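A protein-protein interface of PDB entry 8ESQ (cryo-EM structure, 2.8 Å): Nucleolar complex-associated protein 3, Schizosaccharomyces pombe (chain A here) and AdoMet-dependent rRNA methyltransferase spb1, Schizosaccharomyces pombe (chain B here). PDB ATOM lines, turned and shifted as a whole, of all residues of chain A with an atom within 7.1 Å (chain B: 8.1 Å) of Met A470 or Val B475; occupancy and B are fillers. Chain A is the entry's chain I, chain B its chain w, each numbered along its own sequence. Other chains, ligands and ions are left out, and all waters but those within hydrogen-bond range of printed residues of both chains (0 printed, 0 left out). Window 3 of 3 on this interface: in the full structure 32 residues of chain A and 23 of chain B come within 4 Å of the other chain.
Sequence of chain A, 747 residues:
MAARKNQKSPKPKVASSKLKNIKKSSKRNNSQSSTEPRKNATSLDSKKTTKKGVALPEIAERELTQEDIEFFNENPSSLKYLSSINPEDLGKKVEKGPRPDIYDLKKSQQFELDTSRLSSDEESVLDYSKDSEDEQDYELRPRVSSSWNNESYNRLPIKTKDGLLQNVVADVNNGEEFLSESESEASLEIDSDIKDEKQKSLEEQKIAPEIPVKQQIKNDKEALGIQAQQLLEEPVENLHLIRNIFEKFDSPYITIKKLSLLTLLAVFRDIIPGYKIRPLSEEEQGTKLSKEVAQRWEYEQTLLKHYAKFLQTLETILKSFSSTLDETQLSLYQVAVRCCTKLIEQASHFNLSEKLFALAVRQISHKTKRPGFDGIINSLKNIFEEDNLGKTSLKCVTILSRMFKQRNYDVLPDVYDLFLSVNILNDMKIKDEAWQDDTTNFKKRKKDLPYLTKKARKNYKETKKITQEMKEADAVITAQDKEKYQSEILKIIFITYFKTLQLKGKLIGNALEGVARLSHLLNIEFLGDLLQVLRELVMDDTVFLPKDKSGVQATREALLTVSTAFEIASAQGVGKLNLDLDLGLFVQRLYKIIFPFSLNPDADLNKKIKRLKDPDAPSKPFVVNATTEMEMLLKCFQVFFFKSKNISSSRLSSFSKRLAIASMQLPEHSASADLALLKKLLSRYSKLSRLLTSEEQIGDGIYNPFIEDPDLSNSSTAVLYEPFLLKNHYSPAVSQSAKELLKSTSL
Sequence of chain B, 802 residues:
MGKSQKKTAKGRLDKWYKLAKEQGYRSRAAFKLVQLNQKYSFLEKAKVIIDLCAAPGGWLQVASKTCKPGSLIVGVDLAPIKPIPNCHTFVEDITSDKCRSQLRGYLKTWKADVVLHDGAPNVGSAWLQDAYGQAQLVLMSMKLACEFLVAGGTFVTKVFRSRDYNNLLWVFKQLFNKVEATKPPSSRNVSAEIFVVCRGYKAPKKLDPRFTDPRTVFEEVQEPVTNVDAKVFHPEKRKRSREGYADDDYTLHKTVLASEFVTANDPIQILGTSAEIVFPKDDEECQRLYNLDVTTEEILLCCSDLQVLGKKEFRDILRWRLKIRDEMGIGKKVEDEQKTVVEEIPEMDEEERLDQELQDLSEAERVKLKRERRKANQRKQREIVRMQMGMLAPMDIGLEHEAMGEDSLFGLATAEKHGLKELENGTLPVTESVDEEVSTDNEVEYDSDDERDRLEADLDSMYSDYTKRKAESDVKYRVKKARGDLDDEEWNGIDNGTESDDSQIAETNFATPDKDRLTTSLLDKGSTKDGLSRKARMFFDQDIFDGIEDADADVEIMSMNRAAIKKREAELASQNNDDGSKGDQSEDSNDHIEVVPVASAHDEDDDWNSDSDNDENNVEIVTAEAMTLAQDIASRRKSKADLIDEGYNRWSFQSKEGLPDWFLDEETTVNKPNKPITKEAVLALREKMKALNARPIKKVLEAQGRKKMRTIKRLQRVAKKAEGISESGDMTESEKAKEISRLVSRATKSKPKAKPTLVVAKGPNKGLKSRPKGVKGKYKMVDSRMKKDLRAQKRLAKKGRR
The side-chain carboxylate of Asp B474 lies within salt-bridge range of the side-chain amino group of Lys B476 (3.4 Å).
Val B475 touches Glu A469 (CG1 to O, 3.98 Å). CE of Met A470 touches CG1 of Val B475, 3.6 Å away. Met A470 touches Val B479. Val B475 touches Ala A473 (CG1 to CB, 3.7 Å). Val B479 touches Ala A473 (CG2 to CB, 3.7 Å). CG1 of Val B479 touches OD2 of Asp A474, 3.7 Å away. Lys B476 touches Ile A477 (O to CD1, 3.8 Å). Ile A477 touches Val B479. Lys B480 touches Ile A477.
Met A470 touches just these residues of chain B: Val B475 and Val B479. Of the printed residues of chain A, Val B475 touches Glu A469, Met A470 and Ala A473. Printed residues of chain A within 4 Å of Val B479: Met A470 (3.6 Å), Ala A473 (3.7 Å), Asp A474 (3.7 Å) and Ile A477 (3.7 Å). Printed residues of chain B within 4 Å of Asp A474: Val B479 (3.7 Å) and Arg B483 (2.8 Å). Of the printed residues of chain A, Arg B483 touches Asp A474. Of the printed residues of chain B, Ala A473 touches Val B475 and Val B479. Of the printed residues of chain A, Lys B480 touches Ile A477. Glu B472 touches none of the printed residues of chain A. Lys A464 touches none of the printed residues of chain B. The nearest printed residue of chain A that does not touch Val B475 is Ile A477 (5.7 Å).
Printed residues of chain A that touch a printed residue of chain B: Glu A469, Met A470, Ala A473, Asp A474 and Ile A477. Along chain A the printed residues that touch a printed residue of chain B span positions 469 to 477. Printed residues of chain B that touch a printed residue of chain A: Val B475, Lys B476, Val B479, Lys B480 and Arg B483. Among the printed residues, Asp or Glu carboxylates within 4 Å of a Lys or Arg side-chain nitrogen of the other chain: Asp A474 with Arg B483 (2.8 Å).
The side-chain carboxylate of Asp A474 lies within salt-bridge range of the guanidinium group of Arg B483, at 2.8 Å.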
ATOM      1  N   LYS A 464     -12.108   0.778   2.245  1.00  0.00           N
ATOM      2  CA  LYS A 464     -11.988  -0.657   2.481  1.00  0.00           C
ATOM      3  C   LYS A 464     -13.355  -1.327   2.518  1.00  0.00           C
ATOM      4  O   LYS A 464     -13.526  -2.434   1.992  1.00  0.00           O
ATOM      5  CB  LYS A 464     -11.225  -0.914   3.780  1.00  0.00           C
ATOM      6  CG  LYS A 464     -10.855  -2.368   4.001  1.00  0.00           C
ATOM      7  CD  LYS A 464      -9.961  -2.533   5.219  1.00  0.00           C
ATOM      8  CE  LYS A 464      -9.634  -3.995   5.468  1.00  0.00           C
ATOM      9  NZ  LYS A 464      -8.683  -4.166   6.598  1.00  0.00           N
ATOM     10  N   LYS A 465     -14.340  -0.677   3.141  1.00  0.00           N
ATOM     11  CA  LYS A 465     -15.693  -1.224   3.161  1.00  0.00           C
ATOM     12  C   LYS A 465     -16.275  -1.300   1.754  1.00  0.00           C
ATOM     13  O   LYS A 465     -16.950  -2.272   1.401  1.00  0.00           O
ATOM     14  CB  LYS A 465     -16.586  -0.382   4.072  1.00  0.00           C
ATOM     15  CG  LYS A 465     -16.036  -0.206   5.476  1.00  0.00           C
ATOM     16  CD  LYS A 465     -16.740   0.920   6.211  1.00  0.00           C
ATOM     17  CE  LYS A 465     -15.996   1.294   7.484  1.00  0.00           C
ATOM     18  NZ  LYS A 465     -16.610   2.468   8.161  1.00  0.00           N
ATOM     19  N   ILE A 466     -16.029  -0.273   0.937  1.00  0.00           N
ATOM     20  CA  ILE A 466     -16.522  -0.285  -0.438  1.00  0.00           C
ATOM     21  C   ILE A 466     -15.888  -1.426  -1.223  1.00  0.00           C
ATOM     22  O   ILE A 466     -16.573  -2.148  -1.957  1.00  0.00           O
ATOM     23  CB  ILE A 466     -16.263   1.073  -1.117  1.00  0.00           C
ATOM     24  CG1 ILE A 466     -17.087   2.175  -0.452  1.00  0.00           C
ATOM     25  CG2 ILE A 466     -16.574   0.993  -2.604  1.00  0.00           C
ATOM     26  CD1 ILE A 466     -17.034   3.492  -1.194  1.00  0.00           C
ATOM     27  N   THR A 467     -14.573  -1.608  -1.080  1.00  0.00           N
ATOM     28  CA  THR A 467     -13.883  -2.647  -1.840  1.00  0.00           C
ATOM     29  C   THR A 467     -14.403  -4.032  -1.480  1.00  0.00           C
ATOM     30  O   THR A 467     -14.611  -4.872  -2.363  1.00  0.00           O
ATOM     31  CB  THR A 467     -12.377  -2.564  -1.603  1.00  0.00           C
ATOM     32  OG1 THR A 467     -12.117  -2.491  -0.197  1.00  0.00           O
ATOM     33  CG2 THR A 467     -11.799  -1.335  -2.285  1.00  0.00           C
ATOM     34  N   GLN A 468     -14.618  -4.291  -0.189  1.00  0.00           N
ATOM     35  CA  GLN A 468     -15.165  -5.579   0.225  1.00  0.00           C
ATOM     36  C   GLN A 468     -16.563  -5.784  -0.344  1.00  0.00           C
ATOM     37  O   GLN A 468     -16.897  -6.873  -0.826  1.00  0.00           O
ATOM     38  CB  GLN A 468     -15.183  -5.675   1.750  1.00  0.00           C
ATOM     39  CG  GLN A 468     -15.834  -6.940   2.282  1.00  0.00           C
ATOM     40  CD  GLN A 468     -15.710  -7.068   3.786  1.00  0.00           C
ATOM     41  OE1 GLN A 468     -15.126  -6.210   4.448  1.00  0.00           O
ATOM     42  NE2 GLN A 468     -16.261  -8.144   4.335  1.00  0.00           N
ATOM     43  N   GLU A 469     -17.398  -4.745  -0.291  1.00  0.00           N
ATOM     44  CA  GLU A 469     -18.719  -4.827  -0.904  1.00  0.00           C
ATOM     45  C   GLU A 469     -18.613  -4.946  -2.418  1.00  0.00           C
ATOM     46  O   GLU A 469     -19.392  -5.671  -3.047  1.00  0.00           O
ATOM     47  CB  GLU A 469     -19.552  -3.607  -0.514  1.00  0.00           C
ATOM     48  CG  GLU A 469     -19.881  -3.534   0.966  1.00  0.00           C
ATOM     49  CD  GLU A 469     -20.478  -2.200   1.361  1.00  0.00           C
ATOM     50  OE1 GLU A 469     -20.563  -1.305   0.494  1.00  0.00           O
ATOM     51  OE2 GLU A 469     -20.859  -2.043   2.540  1.00  0.00           O
ATOM     52  N   MET A 470     -17.656  -4.235  -3.022  1.00  0.00           N
ATOM     53  CA  MET A 470     -17.434  -4.362  -4.459  1.00  0.00           C
ATOM     54  C   MET A 470     -17.033  -5.784  -4.828  1.00  0.00           C
ATOM     55  O   MET A 470     -17.518  -6.336  -5.822  1.00  0.00           O
ATOM     56  CB  MET A 470     -16.352  -3.381  -4.914  1.00  0.00           C
ATOM     57  CG  MET A 470     -16.824  -1.996  -5.366  1.00  0.00           C
ATOM     58  SD  MET A 470     -18.422  -1.912  -6.195  1.00  0.00           S
ATOM     59  CE  MET A 470     -19.525  -1.603  -4.817  1.00  0.00           C
ATOM     60  N   LYS A 471     -16.147  -6.391  -4.036  1.00  0.00           N
ATOM     61  CA  LYS A 471     -15.648  -7.725  -4.356  1.00  0.00           C
ATOM     62  C   LYS A 471     -16.761  -8.763  -4.289  1.00  0.00           C
ATOM     63  O   LYS A 471     -16.870  -9.629  -5.166  1.00  0.00           O
ATOM     64  CB  LYS A 471     -14.508  -8.094  -3.407  1.00  0.00           C
ATOM     65  CG  LYS A 471     -13.203  -7.368  -3.688  1.00  0.00           C
ATOM     66  CD  LYS A 471     -12.155  -7.706  -2.640  1.00  0.00           C
ATOM     67  CE  LYS A 471     -10.893  -6.879  -2.825  1.00  0.00           C
ATOM     68  NZ  LYS A 471      -9.916  -7.113  -1.725  1.00  0.00           N
ATOM     69  N   GLU A 472     -17.594  -8.700  -3.249  1.00  0.00           N
ATOM     70  CA  GLU A 472     -18.661  -9.684  -3.095  1.00  0.00           C
ATOM     71  C   GLU A 472     -19.666  -9.589  -4.236  1.00  0.00           C
ATOM     72  O   GLU A 472     -20.093 -10.608  -4.789  1.00  0.00           O
ATOM     73  CB  GLU A 472     -19.359  -9.498  -1.748  1.00  0.00           C
ATOM     74  CG  GLU A 472     -18.494  -9.831  -0.550  1.00  0.00           C
ATOM     75  CD  GLU A 472     -19.296  -9.910   0.733  1.00  0.00           C
ATOM     76  OE1 GLU A 472     -20.520  -9.668   0.683  1.00  0.00           O
ATOM     77  OE2 GLU A 472     -18.703 -10.209   1.790  1.00  0.00           O
ATOM     78  N   ALA A 473     -20.060  -8.366  -4.598  1.00  0.00           N
ATOM     79  CA  ALA A 473     -20.992  -8.190  -5.706  1.00  0.00           C
ATOM     80  C   ALA A 473     -20.354  -8.585  -7.031  1.00  0.00           C
ATOM     81  O   ALA A 473     -21.011  -9.179  -7.893  1.00  0.00           O
ATOM     82  CB  ALA A 473     -21.486  -6.746  -5.754  1.00  0.00           C
ATOM     83  N   ASP A 474     -19.072  -8.257  -7.214  1.00  0.00           N
ATOM     84  CA  ASP A 474     -18.383  -8.634  -8.444  1.00  0.00           C
ATOM     85  C   ASP A 474     -18.299 -10.148  -8.583  1.00  0.00           C
ATOM     86  O   ASP A 474     -18.474 -10.686  -9.681  1.00  0.00           O
ATOM     87  CB  ASP A 474     -16.986  -8.014  -8.476  1.00  0.00           C
ATOM     88  CG  ASP A 474     -16.408  -7.947  -9.878  1.00  0.00           C
ATOM     89  OD1 ASP A 474     -16.358  -8.992 -10.560  1.00  0.00           O
ATOM     90  OD2 ASP A 474     -15.998  -6.845 -10.298  1.00  0.00           O
ATOM     91  N   ALA A 475     -18.034 -10.851  -7.479  1.00  0.00           N
ATOM     92  CA  ALA A 475     -17.951 -12.307  -7.525  1.00  0.00           C
ATOM     93  C   ALA A 475     -19.278 -12.917  -7.961  1.00  0.00           C
ATOM     94  O   ALA A 475     -19.313 -13.826  -8.797  1.00  0.00           O
ATOM     95  CB  ALA A 475     -17.527 -12.851  -6.162  1.00  0.00           C
ATOM     96  N   VAL A 476     -20.384 -12.426  -7.399  1.00  0.00           N
ATOM     97  CA  VAL A 476     -21.702 -12.920  -7.793  1.00  0.00           C
ATOM     98  C   VAL A 476     -21.989 -12.563  -9.245  1.00  0.00           C
ATOM     99  O   VAL A 476     -22.493 -13.386 -10.019  1.00  0.00           O
ATOM    100  CB  VAL A 476     -22.784 -12.369  -6.848  1.00  0.00           C
ATOM    101  CG1 VAL A 476     -24.167 -12.738  -7.353  1.00  0.00           C
ATOM    102  CG2 VAL A 476     -22.568 -12.894  -5.440  1.00  0.00           C
ATOM    103  N   ILE A 477     -21.671 -11.329  -9.637  1.00  0.00           N
ATOM    104  CA  ILE A 477     -21.903 -10.899 -11.012  1.00  0.00           C
ATOM    105  C   ILE A 477     -21.017 -11.681 -11.975  1.00  0.00           C
ATOM    106  O   ILE A 477     -21.444 -12.043 -13.078  1.00  0.00           O
ATOM    107  CB  ILE A 477     -21.691  -9.380 -11.134  1.00  0.00           C
ATOM    108  CG1 ILE A 477     -22.868  -8.634 -10.501  1.00  0.00           C
ATOM    109  CG2 ILE A 477     -21.511  -8.967 -12.586  1.00  0.00           C
ATOM    110  CD1 ILE A 477     -22.764  -7.131 -10.590  1.00  0.00           C
ATOM    111  N   ALA B 471     -28.963   5.758  -9.733  1.00  0.00           N
ATOM    112  CA  ALA B 471     -28.473   4.419 -10.041  1.00  0.00           C
ATOM    113  C   ALA B 471     -27.216   4.070  -9.254  1.00  0.00           C
ATOM    114  O   ALA B 471     -26.951   2.888  -9.017  1.00  0.00           O
ATOM    115  CB  ALA B 471     -28.206   4.290 -11.540  1.00  0.00           C
ATOM    116  N   GLU B 472     -26.433   5.073  -8.847  1.00  0.00           N
ATOM    117  CA  GLU B 472     -25.200   4.805  -8.113  1.00  0.00           C
ATOM    118  C   GLU B 472     -25.460   4.206  -6.739  1.00  0.00           C
ATOM    119  O   GLU B 472     -24.538   3.646  -6.137  1.00  0.00           O
ATOM    120  CB  GLU B 472     -24.376   6.084  -7.962  1.00  0.00           C
ATOM    121  CG  GLU B 472     -23.833   6.638  -9.264  1.00  0.00           C
ATOM    122  CD  GLU B 472     -22.876   5.688  -9.950  1.00  0.00           C
ATOM    123  OE1 GLU B 472     -22.185   4.924  -9.247  1.00  0.00           O
ATOM    124  OE2 GLU B 472     -22.814   5.708 -11.197  1.00  0.00           O
ATOM    125  N   SER B 473     -26.684   4.316  -6.223  1.00  0.00           N
ATOM    126  CA  SER B 473     -27.012   3.692  -4.948  1.00  0.00           C
ATOM    127  C   SER B 473     -27.041   2.173  -5.035  1.00  0.00           C
ATOM    128  O   SER B 473     -27.086   1.511  -3.992  1.00  0.00           O
ATOM    129  CB  SER B 473     -28.358   4.210  -4.443  1.00  0.00           C
ATOM    130  OG  SER B 473     -29.409   3.822  -5.310  1.00  0.00           O
ATOM    131  N   ASP B 474     -27.016   1.611  -6.239  1.00  0.00           N
ATOM    132  CA  ASP B 474     -27.026   0.168  -6.432  1.00  0.00           C
ATOM    133  C   ASP B 474     -25.593  -0.349  -6.417  1.00  0.00           C
ATOM    134  O   ASP B 474     -24.750   0.121  -7.188  1.00  0.00           O
ATOM    135  CB  ASP B 474     -27.714  -0.190  -7.748  1.00  0.00           C
ATOM    136  CG  ASP B 474     -27.807  -1.685  -7.969  1.00  0.00           C
ATOM    137  OD1 ASP B 474     -28.193  -2.403  -7.023  1.00  0.00           O
ATOM    138  OD2 ASP B 474     -27.488  -2.144  -9.085  1.00  0.00           O
ATOM    139  N   VAL B 475     -25.319  -1.310  -5.533  1.00  0.00           N
ATOM    140  CA  VAL B 475     -23.987  -1.906  -5.467  1.00  0.00           C
ATOM    141  C   VAL B 475     -23.667  -2.633  -6.766  1.00  0.00           C
ATOM    142  O   VAL B 475     -22.549  -2.539  -7.289  1.00  0.00           O
ATOM    143  CB  VAL B 475     -23.886  -2.844  -4.250  1.00  0.00           C
ATOM    144  CG1 VAL B 475     -22.547  -3.552  -4.233  1.00  0.00           C
ATOM    145  CG2 VAL B 475     -24.093  -2.062  -2.962  1.00  0.00           C
ATOM    146  N   LYS B 476     -24.644  -3.362  -7.308  1.00  0.00           N
ATOM    147  CA  LYS B 476     -24.439  -4.085  -8.559  1.00  0.00           C
ATOM    148  C   LYS B 476     -24.158  -3.133  -9.715  1.00  0.00           C
ATOM    149  O   LYS B 476     -23.311  -3.419 -10.569  1.00  0.00           O
ATOM    150  CB  LYS B 476     -25.661  -4.950  -8.860  1.00  0.00           C
ATOM    151  CG  LYS B 476     -25.874  -6.081  -7.869  1.00  0.00           C
ATOM    152  CD  LYS B 476     -27.138  -6.866  -8.182  1.00  0.00           C
ATOM    153  CE  LYS B 476     -28.385  -6.042  -7.900  1.00  0.00           C
ATOM    154  NZ  LYS B 476     -28.507  -5.699  -6.456  1.00  0.00           N
ATOM    155  N   TYR B 477     -24.865  -2.001  -9.766  1.00  0.00           N
ATOM    156  CA  TYR B 477     -24.665  -1.052 -10.858  1.00  0.00           C
ATOM    157  C   TYR B 477     -23.248  -0.497 -10.858  1.00  0.00           C
ATOM    158  O   TYR B 477     -22.639  -0.329 -11.922  1.00  0.00           O
ATOM    159  CB  TYR B 477     -25.682   0.084 -10.762  1.00  0.00           C
ATOM    160  CG  TYR B 477     -25.461   1.187 -11.772  1.00  0.00           C
ATOM    161  CD1 TYR B 477     -25.916   1.061 -13.076  1.00  0.00           C
ATOM    162  CD2 TYR B 477     -24.796   2.355 -11.419  1.00  0.00           C
ATOM    163  CE1 TYR B 477     -25.715   2.066 -14.001  1.00  0.00           C
ATOM    164  CE2 TYR B 477     -24.590   3.363 -12.336  1.00  0.00           C
ATOM    165  CZ  TYR B 477     -25.051   3.214 -13.626  1.00  0.00           C
ATOM    166  OH  TYR B 477     -24.849   4.218 -14.543  1.00  0.00           O
ATOM    167  N   ARG B 478     -22.711  -0.190  -9.676  1.00  0.00           N
ATOM    168  CA  ARG B 478     -21.336   0.292  -9.593  1.00  0.00           C
ATOM    169  C   ARG B 478     -20.353  -0.770 -10.070  1.00  0.00           C
ATOM    170  O   ARG B 478     -19.332  -0.447 -10.690  1.00  0.00           O
ATOM    171  CB  ARG B 478     -21.020   0.726  -8.163  1.00  0.00           C
ATOM    172  CG  ARG B 478     -21.682   2.033  -7.763  1.00  0.00           C
ATOM    173  CD  ARG B 478     -21.321   2.436  -6.346  1.00  0.00           C
ATOM    174  NE  ARG B 478     -22.012   1.620  -5.356  1.00  0.00           N
ATOM    175  CZ  ARG B 478     -21.785   1.674  -4.050  1.00  0.00           C
ATOM    176  NH1 ARG B 478     -20.875   2.487  -3.540  1.00  0.00           N
ATOM    177  NH2 ARG B 478     -22.489   0.893  -3.237  1.00  0.00           N
ATOM    178  N   VAL B 479     -20.640  -2.042  -9.784  1.00  0.00           N
ATOM    179  CA  VAL B 479     -19.814  -3.125 -10.312  1.00  0.00           C
ATOM    180  C   VAL B 479     -19.906  -3.172 -11.831  1.00  0.00           C
ATOM    181  O   VAL B 479     -18.898  -3.356 -12.524  1.00  0.00           O
ATOM    182  CB  VAL B 479     -20.220  -4.468  -9.678  1.00  0.00           C
ATOM    183  CG1 VAL B 479     -19.451  -5.611 -10.319  1.00  0.00           C
ATOM    184  CG2 VAL B 479     -19.982  -4.439  -8.180  1.00  0.00           C
ATOM    185  N   LYS B 480     -21.116  -3.012 -12.373  1.00  0.00           N
ATOM    186  CA  LYS B 480     -21.297  -3.064 -13.821  1.00  0.00           C
ATOM    187  C   LYS B 480     -20.523  -1.949 -14.515  1.00  0.00           C
ATOM    188  O   LYS B 480     -19.872  -2.177 -15.541  1.00  0.00           O
ATOM    189  CB  LYS B 480     -22.783  -2.979 -14.167  1.00  0.00           C
ATOM    190  CG  LYS B 480     -23.616  -4.137 -13.652  1.00  0.00           C
ATOM    191  CD  LYS B 480     -23.309  -5.417 -14.404  1.00  0.00           C
ATOM    192  CE  LYS B 480     -24.127  -6.579 -13.870  1.00  0.00           C
ATOM    193  NZ  LYS B 480     -25.581  -6.404 -14.136  1.00  0.00           N
ATOM    194  N   LYS B 481     -20.585  -0.732 -13.972  1.00  0.00           N
ATOM    195  CA  LYS B 481     -19.853   0.376 -14.576  1.00  0.00           C
ATOM    196  C   LYS B 481     -18.351   0.181 -14.434  1.00  0.00           C
ATOM    197  O   LYS B 481     -17.575   0.625 -15.288  1.00  0.00           O
ATOM    198  CB  LYS B 481     -20.287   1.702 -13.955  1.00  0.00           C
ATOM    199  CG  LYS B 481     -21.776   2.036 -14.089  1.00  0.00           C
ATOM    200  CD  LYS B 481     -22.253   2.112 -15.538  1.00  0.00           C
ATOM    201  CE  LYS B 481     -22.945   0.826 -15.984  1.00  0.00           C
ATOM    202  NZ  LYS B 481     -23.383   0.881 -17.405  1.00  0.00           N
ATOM    203  N   ALA B 482     -17.919  -0.473 -13.353  1.00  0.00           N
ATOM    204  CA  ALA B 482     -16.507  -0.804 -13.208  1.00  0.00           C
ATOM    205  C   ALA B 482     -16.062  -1.813 -14.256  1.00  0.00           C
ATOM    206  O   ALA B 482     -14.916  -1.767 -14.716  1.00  0.00           O
ATOM    207  CB  ALA B 482     -16.232  -1.338 -11.802  1.00  0.00           C
ATOM    208  N   ARG B 483     -16.945  -2.727 -14.642  1.00  0.00           N
ATOM    209  CA  ARG B 483     -16.616  -3.744 -15.632  1.00  0.00           C
ATOM    210  C   ARG B 483     -17.300  -3.455 -16.965  1.00  0.00           C
ATOM    211  O   ARG B 483     -17.298  -2.321 -17.443  1.00  0.00           O
ATOM    212  CB  ARG B 483     -17.019  -5.129 -15.127  1.00  0.00           C
ATOM    213  CG  ARG B 483     -16.297  -5.560 -13.862  1.00  0.00           C
ATOM    214  CD  ARG B 483     -16.650  -6.988 -13.489  1.00  0.00           C
ATOM    215  NE  ARG B 483     -16.054  -7.952 -14.405  1.00  0.00           N
ATOM    216  CZ  ARG B 483     -16.127  -9.268 -14.258  1.00  0.00           C
ATOM    217  NH1 ARG B 483     -16.781  -9.815 -13.247  1.00  0.00           N
ATOM    218  NH2 ARG B 483     -15.530 -10.055 -15.150  1.00  0.00           N
